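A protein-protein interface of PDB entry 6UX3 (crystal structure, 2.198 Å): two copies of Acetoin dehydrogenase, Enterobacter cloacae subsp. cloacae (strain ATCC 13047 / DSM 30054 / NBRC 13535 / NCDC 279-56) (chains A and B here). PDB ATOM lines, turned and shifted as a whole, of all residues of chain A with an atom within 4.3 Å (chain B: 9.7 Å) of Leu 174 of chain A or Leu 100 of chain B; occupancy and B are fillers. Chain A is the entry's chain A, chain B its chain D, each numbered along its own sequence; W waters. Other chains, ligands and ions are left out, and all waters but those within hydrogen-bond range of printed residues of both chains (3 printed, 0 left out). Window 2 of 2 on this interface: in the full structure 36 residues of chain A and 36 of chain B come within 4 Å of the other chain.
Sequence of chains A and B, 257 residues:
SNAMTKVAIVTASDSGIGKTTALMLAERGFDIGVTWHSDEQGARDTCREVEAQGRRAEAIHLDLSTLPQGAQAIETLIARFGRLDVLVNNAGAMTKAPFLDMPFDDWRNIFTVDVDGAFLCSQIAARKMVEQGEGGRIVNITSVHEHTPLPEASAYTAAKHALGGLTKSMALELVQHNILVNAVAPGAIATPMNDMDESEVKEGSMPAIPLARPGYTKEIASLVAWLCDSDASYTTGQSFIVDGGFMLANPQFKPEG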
ATOM      1  N   GLN A 123      19.921  18.499 -17.011  1.00  0.00           N
ATOM      2  CA  GLN A 123      20.980  19.302 -16.404  1.00  0.00           C
ATOM      3  C   GLN A 123      20.785  20.781 -16.702  1.00  0.00           C
ATOM      4  O   GLN A 123      20.858  21.624 -15.801  1.00  0.00           O
ATOM      5  CB  GLN A 123      22.344  18.847 -16.919  1.00  0.00           C
ATOM      6  CG  GLN A 123      23.014  17.773 -16.101  1.00  0.00           C
ATOM      7  CD  GLN A 123      24.422  17.499 -16.586  1.00  0.00           C
ATOM      8  OE1 GLN A 123      24.708  17.599 -17.780  1.00  0.00           O
ATOM      9  NE2 GLN A 123      25.313  17.163 -15.662  1.00  0.00           N
ATOM     10  N   ALA A 126      17.637  21.981 -14.859  1.00  0.00           N
ATOM     11  CA  ALA A 126      17.766  22.026 -13.405  1.00  0.00           C
ATOM     12  C   ALA A 126      18.609  23.213 -12.956  1.00  0.00           C
ATOM     13  O   ALA A 126      18.299  23.852 -11.944  1.00  0.00           O
ATOM     14  CB  ALA A 126      18.367  20.720 -12.895  1.00  0.00           C
ATOM     15  N   ARG A 127      19.687  23.512 -13.690  1.00  0.00           N
ATOM     16  CA  ARG A 127      20.508  24.680 -13.380  1.00  0.00           C
ATOM     17  C   ARG A 127      19.664  25.945 -13.336  1.00  0.00           C
ATOM     18  O   ARG A 127      19.672  26.679 -12.340  1.00  0.00           O
ATOM     19  CB  ARG A 127      21.629  24.828 -14.411  1.00  0.00           C
ATOM     20  CG  ARG A 127      22.719  23.770 -14.324  1.00  0.00           C
ATOM     21  CD  ARG A 127      23.498  23.700 -15.629  1.00  0.00           C
ATOM     22  NE  ARG A 127      24.358  22.524 -15.698  1.00  0.00           N
ATOM     23  CZ  ARG A 127      24.799  21.992 -16.834  1.00  0.00           C
ATOM     24  NH1 ARG A 127      24.456  22.530 -17.996  1.00  0.00           N
ATOM     25  NH2 ARG A 127      25.575  20.916 -16.809  1.00  0.00           N
ATOM     26  N   MET A 170      17.850  12.155  -9.764  1.00  0.00           N
ATOM     27  CA  MET A 170      17.550  13.575  -9.906  1.00  0.00           C
ATOM     28  C   MET A 170      16.581  14.048  -8.833  1.00  0.00           C
ATOM     29  O   MET A 170      16.756  15.132  -8.264  1.00  0.00           O
ATOM     30  CB  MET A 170      16.972  13.851 -11.291  1.00  0.00           C
ATOM     31  CG  MET A 170      17.966  13.754 -12.426  1.00  0.00           C
ATOM     32  SD  MET A 170      17.149  13.985 -14.017  1.00  0.00           S
ATOM     33  CE  MET A 170      16.075  15.366 -13.650  1.00  0.00           C
ATOM     34  N   ALA A 171      15.548  13.254  -8.547  1.00  0.00           N
ATOM     35  CA  ALA A 171      14.555  13.685  -7.569  1.00  0.00           C
ATOM     36  C   ALA A 171      15.168  13.834  -6.187  1.00  0.00           C
ATOM     37  O   ALA A 171      14.780  14.728  -5.424  1.00  0.00           O
ATOM     38  CB  ALA A 171      13.390  12.699  -7.527  1.00  0.00           C
ATOM     39  N   LEU A 172      16.134  12.980  -5.855  1.00  0.00           N
ATOM     40  CA  LEU A 172      16.761  13.040  -4.543  1.00  0.00           C
ATOM     41  C   LEU A 172      17.731  14.213  -4.430  1.00  0.00           C
ATOM     42  O   LEU A 172      17.743  14.909  -3.411  1.00  0.00           O
ATOM     43  CB  LEU A 172      17.469  11.717  -4.250  1.00  0.00           C
ATOM     44  CG  LEU A 172      17.957  11.514  -2.815  1.00  0.00           C
ATOM     45  CD1 LEU A 172      16.804  11.575  -1.820  1.00  0.00           C
ATOM     46  CD2 LEU A 172      18.703  10.193  -2.697  1.00  0.00           C
ATOM     47  N   GLU A 173      18.540  14.460  -5.468  1.00  0.00           N
ATOM     48  CA  GLU A 173      19.548  15.516  -5.399  1.00  0.00           C
ATOM     49  C   GLU A 173      18.967  16.911  -5.573  1.00  0.00           C
ATOM     50  O   GLU A 173      19.607  17.887  -5.166  1.00  0.00           O
ATOM     51  CB  GLU A 173      20.636  15.299  -6.455  1.00  0.00           C
ATOM     52  CG  GLU A 173      21.510  14.078  -6.225  1.00  0.00           C
ATOM     53  CD  GLU A 173      22.783  14.114  -7.050  1.00  0.00           C
ATOM     54  OE1 GLU A 173      23.291  15.226  -7.314  1.00  0.00           O
ATOM     55  OE2 GLU A 173      23.276  13.034  -7.435  1.00  0.00           O
ATOM     56  N   LEU A 174      17.784  17.032  -6.165  1.00  0.00           N
ATOM     57  CA  LEU A 174      17.165  18.326  -6.412  1.00  0.00           C
ATOM     58  C   LEU A 174      16.049  18.645  -5.428  1.00  0.00           C
ATOM     59  O   LEU A 174      15.442  19.717  -5.529  1.00  0.00           O
ATOM     60  CB  LEU A 174      16.626  18.381  -7.844  1.00  0.00           C
ATOM     61  CG  LEU A 174      17.667  18.192  -8.946  1.00  0.00           C
ATOM     62  CD1 LEU A 174      16.998  18.184 -10.307  1.00  0.00           C
ATOM     63  CD2 LEU A 174      18.729  19.287  -8.866  1.00  0.00           C
ATOM     64  N   VAL A 175      15.775  17.752  -4.472  1.00  0.00           N
ATOM     65  CA  VAL A 175      14.654  17.953  -3.558  1.00  0.00           C
ATOM     66  C   VAL A 175      14.867  19.187  -2.684  1.00  0.00           C
ATOM     67  O   VAL A 175      13.899  19.802  -2.219  1.00  0.00           O
ATOM     68  CB  VAL A 175      14.431  16.685  -2.710  1.00  0.00           C
ATOM     69  CG1 VAL A 175      15.546  16.513  -1.675  1.00  0.00           C
ATOM     70  CG2 VAL A 175      13.070  16.730  -2.040  1.00  0.00           C
ATOM     71  N   GLN A 176      16.121  19.575  -2.449  1.00  0.00           N
ATOM     72  CA  GLN A 176      16.378  20.772  -1.656  1.00  0.00           C
ATOM     73  C   GLN A 176      15.923  22.033  -2.382  1.00  0.00           C
ATOM     74  O   GLN A 176      15.476  22.988  -1.738  1.00  0.00           O
ATOM     75  CB  GLN A 176      17.863  20.852  -1.311  1.00  0.00           C
ATOM     76  CG  GLN A 176      18.770  20.488  -2.476  1.00  0.00           C
ATOM     77  CD  GLN A 176      20.241  20.569  -2.125  1.00  0.00           C
ATOM     78  OE1 GLN A 176      20.640  21.315  -1.231  1.00  0.00           O
ATOM     79  NE2 GLN A 176      21.057  19.793  -2.830  1.00  0.00           N
ATOM     80  N   HIS A 177      16.014  22.050  -3.710  1.00  0.00           N
ATOM     81  CA  HIS A 177      15.609  23.196  -4.513  1.00  0.00           C
ATOM     82  C   HIS A 177      14.135  23.152  -4.904  1.00  0.00           C
ATOM     83  O   HIS A 177      13.701  23.963  -5.731  1.00  0.00           O
ATOM     84  CB  HIS A 177      16.476  23.288  -5.770  1.00  0.00           C
ATOM     85  CG  HIS A 177      17.944  23.225  -5.493  1.00  0.00           C
ATOM     86  ND1 HIS A 177      18.673  24.320  -5.082  1.00  0.00           N
ATOM     87  CD2 HIS A 177      18.821  22.195  -5.567  1.00  0.00           C
ATOM     88  CE1 HIS A 177      19.936  23.968  -4.914  1.00  0.00           C
ATOM     89  NE2 HIS A 177      20.052  22.684  -5.202  1.00  0.00           N
ATOM     90  N   ASN A 178      13.363  22.224  -4.337  1.00  0.00           N
ATOM     91  CA  ASN A 178      11.947  22.063  -4.667  1.00  0.00           C
ATOM     92  C   ASN A 178      11.746  21.794  -6.159  1.00  0.00           C
ATOM     93  O   ASN A 178      10.776  22.252  -6.767  1.00  0.00           O
ATOM     94  CB  ASN A 178      11.132  23.279  -4.220  1.00  0.00           C
ATOM     95  CG  ASN A 178       9.659  22.969  -4.090  1.00  0.00           C
ATOM     96  OD1 ASN A 178       8.811  23.694  -4.610  1.00  0.00           O
ATOM     97  ND2 ASN A 178       9.345  21.876  -3.403  1.00  0.00           N
ATOM     98  N   ILE A 179      12.681  21.065  -6.756  1.00  0.00           N
ATOM     99  CA  ILE A 179      12.561  20.598  -8.132  1.00  0.00           C
ATOM    100  C   ILE A 179      12.123  19.141  -8.069  1.00  0.00           C
ATOM    101  O   ILE A 179      12.908  18.261  -7.695  1.00  0.00           O
ATOM    102  CB  ILE A 179      13.872  20.757  -8.912  1.00  0.00           C
ATOM    103  CG1 ILE A 179      14.307  22.220  -8.945  1.00  0.00           C
ATOM    104  CG2 ILE A 179      13.711  20.232 -10.331  1.00  0.00           C
ATOM    105  CD1 ILE A 179      15.709  22.414  -9.485  1.00  0.00           C
ATOM    106  N   VAL A 181      10.959  15.612  -9.578  1.00  0.00           N
ATOM    107  CA  VAL A 181      11.293  14.841 -10.768  1.00  0.00           C
ATOM    108  C   VAL A 181      10.558  13.511 -10.698  1.00  0.00           C
ATOM    109  O   VAL A 181      10.728  12.748  -9.738  1.00  0.00           O
ATOM    110  CB  VAL A 181      12.806  14.621 -10.899  1.00  0.00           C
ATOM    111  CG1 VAL A 181      13.113  13.917 -12.200  1.00  0.00           C
ATOM    112  CG2 VAL A 181      13.560  15.947 -10.798  1.00  0.00           C
ATOM    113  N   ALA B  97      29.753  11.733  -8.316  1.00  0.00           N
ATOM    114  CA  ALA B  97      29.784  12.971  -9.084  1.00  0.00           C
ATOM    115  C   ALA B  97      28.427  13.660  -9.011  1.00  0.00           C
ATOM    116  O   ALA B  97      27.415  13.076  -9.418  1.00  0.00           O
ATOM    117  CB  ALA B  97      30.167  12.700 -10.538  1.00  0.00           C
ATOM    118  N   PRO B  98      28.364  14.890  -8.496  1.00  0.00           N
ATOM    119  CA  PRO B  98      27.085  15.607  -8.441  1.00  0.00           C
ATOM    120  C   PRO B  98      26.441  15.734  -9.815  1.00  0.00           C
ATOM    121  O   PRO B  98      27.118  15.777 -10.845  1.00  0.00           O
ATOM    122  CB  PRO B  98      27.473  16.978  -7.878  1.00  0.00           C
ATOM    123  CG  PRO B  98      28.704  16.706  -7.079  1.00  0.00           C
ATOM    124  CD  PRO B  98      29.446  15.641  -7.834  1.00  0.00           C
ATOM    125  N   PHE B  99      25.109  15.808  -9.814  1.00  0.00           N
ATOM    126  CA  PHE B  99      24.343  15.748 -11.055  1.00  0.00           C
ATOM    127  C   PHE B  99      24.432  17.041 -11.859  1.00  0.00           C
ATOM    128  O   PHE B  99      24.548  17.000 -13.089  1.00  0.00           O
ATOM    129  CB  PHE B  99      22.881  15.424 -10.746  1.00  0.00           C
ATOM    130  CG  PHE B  99      21.928  15.803 -11.847  1.00  0.00           C
ATOM    131  CD1 PHE B  99      21.826  15.030 -12.993  1.00  0.00           C
ATOM    132  CD2 PHE B  99      21.123  16.927 -11.729  1.00  0.00           C
ATOM    133  CE1 PHE B  99      20.952  15.373 -14.002  1.00  0.00           C
ATOM    134  CE2 PHE B  99      20.242  17.279 -12.740  1.00  0.00           C
ATOM    135  CZ  PHE B  99      20.156  16.503 -13.876  1.00  0.00           C
ATOM    136  N   LEU B 100      24.369  18.192 -11.186  1.00  0.00           N
ATOM    137  CA  LEU B 100      24.202  19.458 -11.897  1.00  0.00           C
ATOM    138  C   LEU B 100      25.380  19.746 -12.817  1.00  0.00           C
ATOM    139  O   LEU B 100      25.195  20.261 -13.927  1.00  0.00           O
ATOM    140  CB  LEU B 100      24.012  20.598 -10.896  1.00  0.00           C
ATOM    141  CG  LEU B 100      22.671  20.625 -10.160  1.00  0.00           C
ATOM    142  CD1 LEU B 100      22.680  21.606  -8.988  1.00  0.00           C
ATOM    143  CD2 LEU B 100      21.550  20.957 -11.132  1.00  0.00           C
ATOM    144  N   ASP B 101      26.595  19.406 -12.387  1.00  0.00           N
ATOM    145  CA  ASP B 101      27.807  19.797 -13.098  1.00  0.00           C
ATOM    146  C   ASP B 101      28.606  18.599 -13.600  1.00  0.00           C
ATOM    147  O   ASP B 101      29.797  18.739 -13.893  1.00  0.00           O
ATOM    148  CB  ASP B 101      28.682  20.675 -12.201  1.00  0.00           C
ATOM    149  CG  ASP B 101      27.926  21.863 -11.629  1.00  0.00           C
ATOM    150  OD1 ASP B 101      27.220  22.550 -12.398  1.00  0.00           O
ATOM    151  OD2 ASP B 101      28.033  22.106 -10.407  1.00  0.00           O
ATOM    152  N   MET B 102      27.989  17.429 -13.709  1.00  0.00           N
ATOM    153  CA  MET B 102      28.740  16.253 -14.131  1.00  0.00           C
ATOM    154  C   MET B 102      29.052  16.342 -15.621  1.00  0.00           C
ATOM    155  O   MET B 102      28.144  16.590 -16.425  1.00  0.00           O
ATOM    156  CB  MET B 102      27.971  14.972 -13.833  1.00  0.00           C
ATOM    157  CG  MET B 102      28.784  13.720 -14.100  1.00  0.00           C
ATOM    158  SD  MET B 102      27.845  12.189 -13.927  1.00  0.00           S
ATOM    159  CE  MET B 102      29.177  10.996 -14.009  1.00  0.00           C
ATOM    160  N   PRO B 103      30.311  16.166 -16.024  1.00  0.00           N
ATOM    161  CA  PRO B 103      30.644  16.211 -17.452  1.00  0.00           C
ATOM    162  C   PRO B 103      30.002  15.062 -18.211  1.00  0.00           C
ATOM    163  O   PRO B 103      29.787  13.974 -17.673  1.00  0.00           O
ATOM    164  CB  PRO B 103      32.174  16.104 -17.467  1.00  0.00           C
ATOM    165  CG  PRO B 103      32.600  16.545 -16.110  1.00  0.00           C
ATOM    166  CD  PRO B 103      31.513  16.098 -15.177  1.00  0.00           C
ATOM    167  N   PHE B 104      29.713  15.314 -19.490  1.00  0.00           N
ATOM    168  CA  PHE B 104      28.995  14.326 -20.289  1.00  0.00           C
ATOM    169  C   PHE B 104      29.836  13.083 -20.544  1.00  0.00           C
ATOM    170  O   PHE B 104      29.287  11.985 -20.689  1.00  0.00           O
ATOM    171  CB  PHE B 104      28.543  14.947 -21.611  1.00  0.00           C
ATOM    172  CG  PHE B 104      27.745  14.015 -22.478  1.00  0.00           C
ATOM    173  CD1 PHE B 104      26.625  13.368 -21.978  1.00  0.00           C
ATOM    174  CD2 PHE B 104      28.101  13.797 -23.798  1.00  0.00           C
ATOM    175  CE1 PHE B 104      25.883  12.513 -22.776  1.00  0.00           C
ATOM    176  CE2 PHE B 104      27.363  12.944 -24.603  1.00  0.00           C
ATOM    177  CZ  PHE B 104      26.251  12.304 -24.091  1.00  0.00           C
ATOM    178  N   TRP B 107      29.783  10.766 -17.470  1.00  0.00           N
ATOM    179  CA  TRP B 107      28.512  10.053 -17.492  1.00  0.00           C
ATOM    180  C   TRP B 107      28.576   8.863 -18.440  1.00  0.00           C
ATOM    181  O   TRP B 107      28.192   7.745 -18.080  1.00  0.00           O
ATOM    182  CB  TRP B 107      27.395  11.024 -17.886  1.00  0.00           C
ATOM    183  CG  TRP B 107      26.137  10.379 -18.390  1.00  0.00           C
ATOM    184  CD1 TRP B 107      25.861  10.015 -19.676  1.00  0.00           C
ATOM    185  CD2 TRP B 107      24.972  10.047 -17.623  1.00  0.00           C
ATOM    186  NE1 TRP B 107      24.604   9.465 -19.757  1.00  0.00           N
ATOM    187  CE2 TRP B 107      24.037   9.474 -18.510  1.00  0.00           C
ATOM    188  CE3 TRP B 107      24.632  10.173 -16.273  1.00  0.00           C
ATOM    189  CZ2 TRP B 107      22.782   9.026 -18.090  1.00  0.00           C
ATOM    190  CZ3 TRP B 107      23.386   9.727 -15.856  1.00  0.00           C
ATOM    191  CH2 TRP B 107      22.477   9.160 -16.763  1.00  0.00           C
ATOM    192  N   PRO B 151      22.899   8.740  -3.227  1.00  0.00           N
ATOM    193  CA  PRO B 151      23.135  10.188  -3.302  1.00  0.00           C
ATOM    194  C   PRO B 151      24.485  10.513  -3.924  1.00  0.00           C
ATOM    195  O   PRO B 151      25.496   9.872  -3.628  1.00  0.00           O
ATOM    196  CB  PRO B 151      23.071  10.631  -1.837  1.00  0.00           C
ATOM    197  CG  PRO B 151      22.201   9.618  -1.183  1.00  0.00           C
ATOM    198  CD  PRO B 151      22.543   8.312  -1.865  1.00  0.00           C
ATOM    199  N   GLU B 152      24.480  11.518  -4.805  1.00  0.00           N
ATOM    200  CA  GLU B 152      25.672  12.020  -5.494  1.00  0.00           C
ATOM    201  C   GLU B 152      26.271  10.993  -6.446  1.00  0.00           C
ATOM    202  O   GLU B 152      27.460  11.055  -6.766  1.00  0.00           O
ATOM    203  CB  GLU B 152      26.740  12.508  -4.505  1.00  0.00           C
ATOM    204  CG  GLU B 152      26.451  13.871  -3.914  1.00  0.00           C
ATOM    205  CD  GLU B 152      25.294  13.844  -2.937  1.00  0.00           C
ATOM    206  OE1 GLU B 152      25.371  13.070  -1.959  1.00  0.00           O
ATOM    207  OE2 GLU B 152      24.308  14.581  -3.152  1.00  0.00           O
ATOM    208  N   ALA B 153      25.460  10.055  -6.919  1.00  0.00           N
ATOM    209  CA  ALA B 153      25.927   9.033  -7.843  1.00  0.00           C
ATOM    210  C   ALA B 153      24.798   8.673  -8.809  1.00  0.00           C
ATOM    211  O   ALA B 153      24.360   7.528  -8.906  1.00  0.00           O
ATOM    212  CB  ALA B 153      26.442   7.819  -7.075  1.00  0.00           C
ATOM    213  N   SER B 154      24.315   9.671  -9.554  1.00  0.00           N
ATOM    214  CA  SER B 154      23.204   9.442 -10.474  1.00  0.00           C
ATOM    215  C   SER B 154      23.611   8.551 -11.642  1.00  0.00           C
ATOM    216  O   SER B 154      22.824   7.710 -12.088  1.00  0.00           O
ATOM    217  CB  SER B 154      22.655  10.777 -10.982  1.00  0.00           C
ATOM    218  OG  SER B 154      23.646  11.532 -11.652  1.00  0.00           O
ATOM    219  N   ALA B 155      24.834   8.721 -12.158  1.00  0.00           N
ATOM    220  CA  ALA B 155      25.279   7.904 -13.285  1.00  0.00           C
ATOM    221  C   ALA B 155      25.466   6.451 -12.874  1.00  0.00           C
ATOM    222  O   ALA B 155      25.112   5.532 -13.625  1.00  0.00           O
ATOM    223  CB  ALA B 155      26.581   8.461 -13.863  1.00  0.00           C
HETATM  224  O   HOH W   1      27.522  16.998 -18.984  1.00  0.00           O
HETATM  225  O   HOH W   2      23.698  18.125  -8.116  1.00  0.00           O
HETATM  226  O   HOH W   3      24.863  12.594  -9.567  1.00  0.00           O
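Printed residues of chain B that touch a printed residue of chain A: Pro 98, Phe 99, Leu 100, Met 102, Pro 151, Glu 152 and Ala 153. Of the 14 printed residues of chain A, 7 touch a printed residue of chain B. Hydrophobic or aromatic side chains of chain A that line the printed part of chain B: Ala 126, Met 170, Leu 172 and Leu 174. Among the printed residues, 13 pairs touch across the chains.
No position is printed for both chains. Of the 13 pairs that touch across the chains among the printed residues, none has its exchanged pair printed and touching as well.
NE2 of Gln 123 of chain A sits at hydrogen-bond distance from O of Phe 99 of chain B (2.7 Å). The side-chain amide nitrogen (NE2) of Gln 123 of chain A sits at hydrogen-bond distance from the backbone carbonyl oxygen (O) of Met 102 of chain B (3.0 Å). The guanidinium group (NH2) of Arg 127 of chain A is in hydrogen-bond range of the backbone carbonyl oxygen (O) of Leu 100 of chain B (3.0 Å). The side-chain carboxylate (OE1) of Glu 173 of chain A sits at hydrogen-bond distance from the backbone NH (N) of Phe 99 of chain B (3.1 Å). The side-chain carboxylate of Glu 173 of chain A sits close to the backbone NH of Glu 152 of chain B, 3.3 Å away.
Among the printed residues, pairs that only touch across the chains: Gln 123 of chain A with Leu 100 of chain B, Ala 126 of chain A with Phe 99 of chain B, Ala 126 of chain A with Leu 100 of chain B, Met 170 of chain A with Phe 99 of chain B, Leu 172 of chain A with Pro 151 of chain B, Glu 173 of chain A with Pro 98 of chain B, Glu 173 of chain A with Ala 153 of chain B and Leu 174 of chain A with Leu 100 of chain B.
NE2 of Gln 176 of chain A lies within hydrogen-bond range of O of Glu 173 of chain A (3.3 Å). O of Leu 174 of chain A sits at hydrogen-bond distance from N of Ile 179 of chain A, at 3.3 Å. The backbone carbonyl oxygen of Glu 152 of chain B lies within hydrogen-bond range of the backbone NH of Ala 97 of chain B (2.8 Å).
Printed residues of chain B within 4 Å of Leu 174 of chain A: Leu 100. Printed residues of chain A within 4 Å of Leu 100 of chain B: Gln 123 (3.6 Å), Ala 126 (3.6 Å), Arg 127 (3.0 Å) and Leu 174 (3.99 Å). Ala 126 of chain A touches just these residues of chain B: Phe 99 and Leu 100. Val 175 of chain A touches none of the printed residues of chain B. No residue of chain B comes within 4 Å of His 177 of chain A. No residue of chain B comes within 4 Å of Ile 179 of chain A. Printed residues of chain A within 4 Å of Ala 153 of chain B: Glu 173. Of the printed residues of chain A, Pro 151 of chain B touches Leu 172 (3.9 Å). Printed residues of chain A within 4 Å of Met 102 of chain B: Gln 123. The nearest printed residue of chain B that does not touch Leu 174 of chain A is Phe 99 of chain B (4.2 Å). The nearest printed residue of chain A that does not touch Leu 100 of chain B is His 177 of chain A (4.7 Å).
Water W3 lies within hydrogen-bond range of O of Ala 97 of chain B (2.6 Å), OG of Ser 154 of chain B (2.6 Å), OE2 of Glu 173 of chain A (2.7 Å) and N of Phe 99 of chain B (3.2 Å). Water W1 lies within hydrogen-bond range of the backbone carbonyl oxygen (O) of Met 102 of chain B, the backbone NH (N) of Phe 104 of chain B and the side-chain amide oxygen (OE1) of Gln 123 of chain A. Water W2 lies within hydrogen-bond range of OE1 of Glu 173 of chain A (3.0 Å), N of Leu 100 of chain B (3.1 Å) and N of Phe 99 of chain B (3.2 Å).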
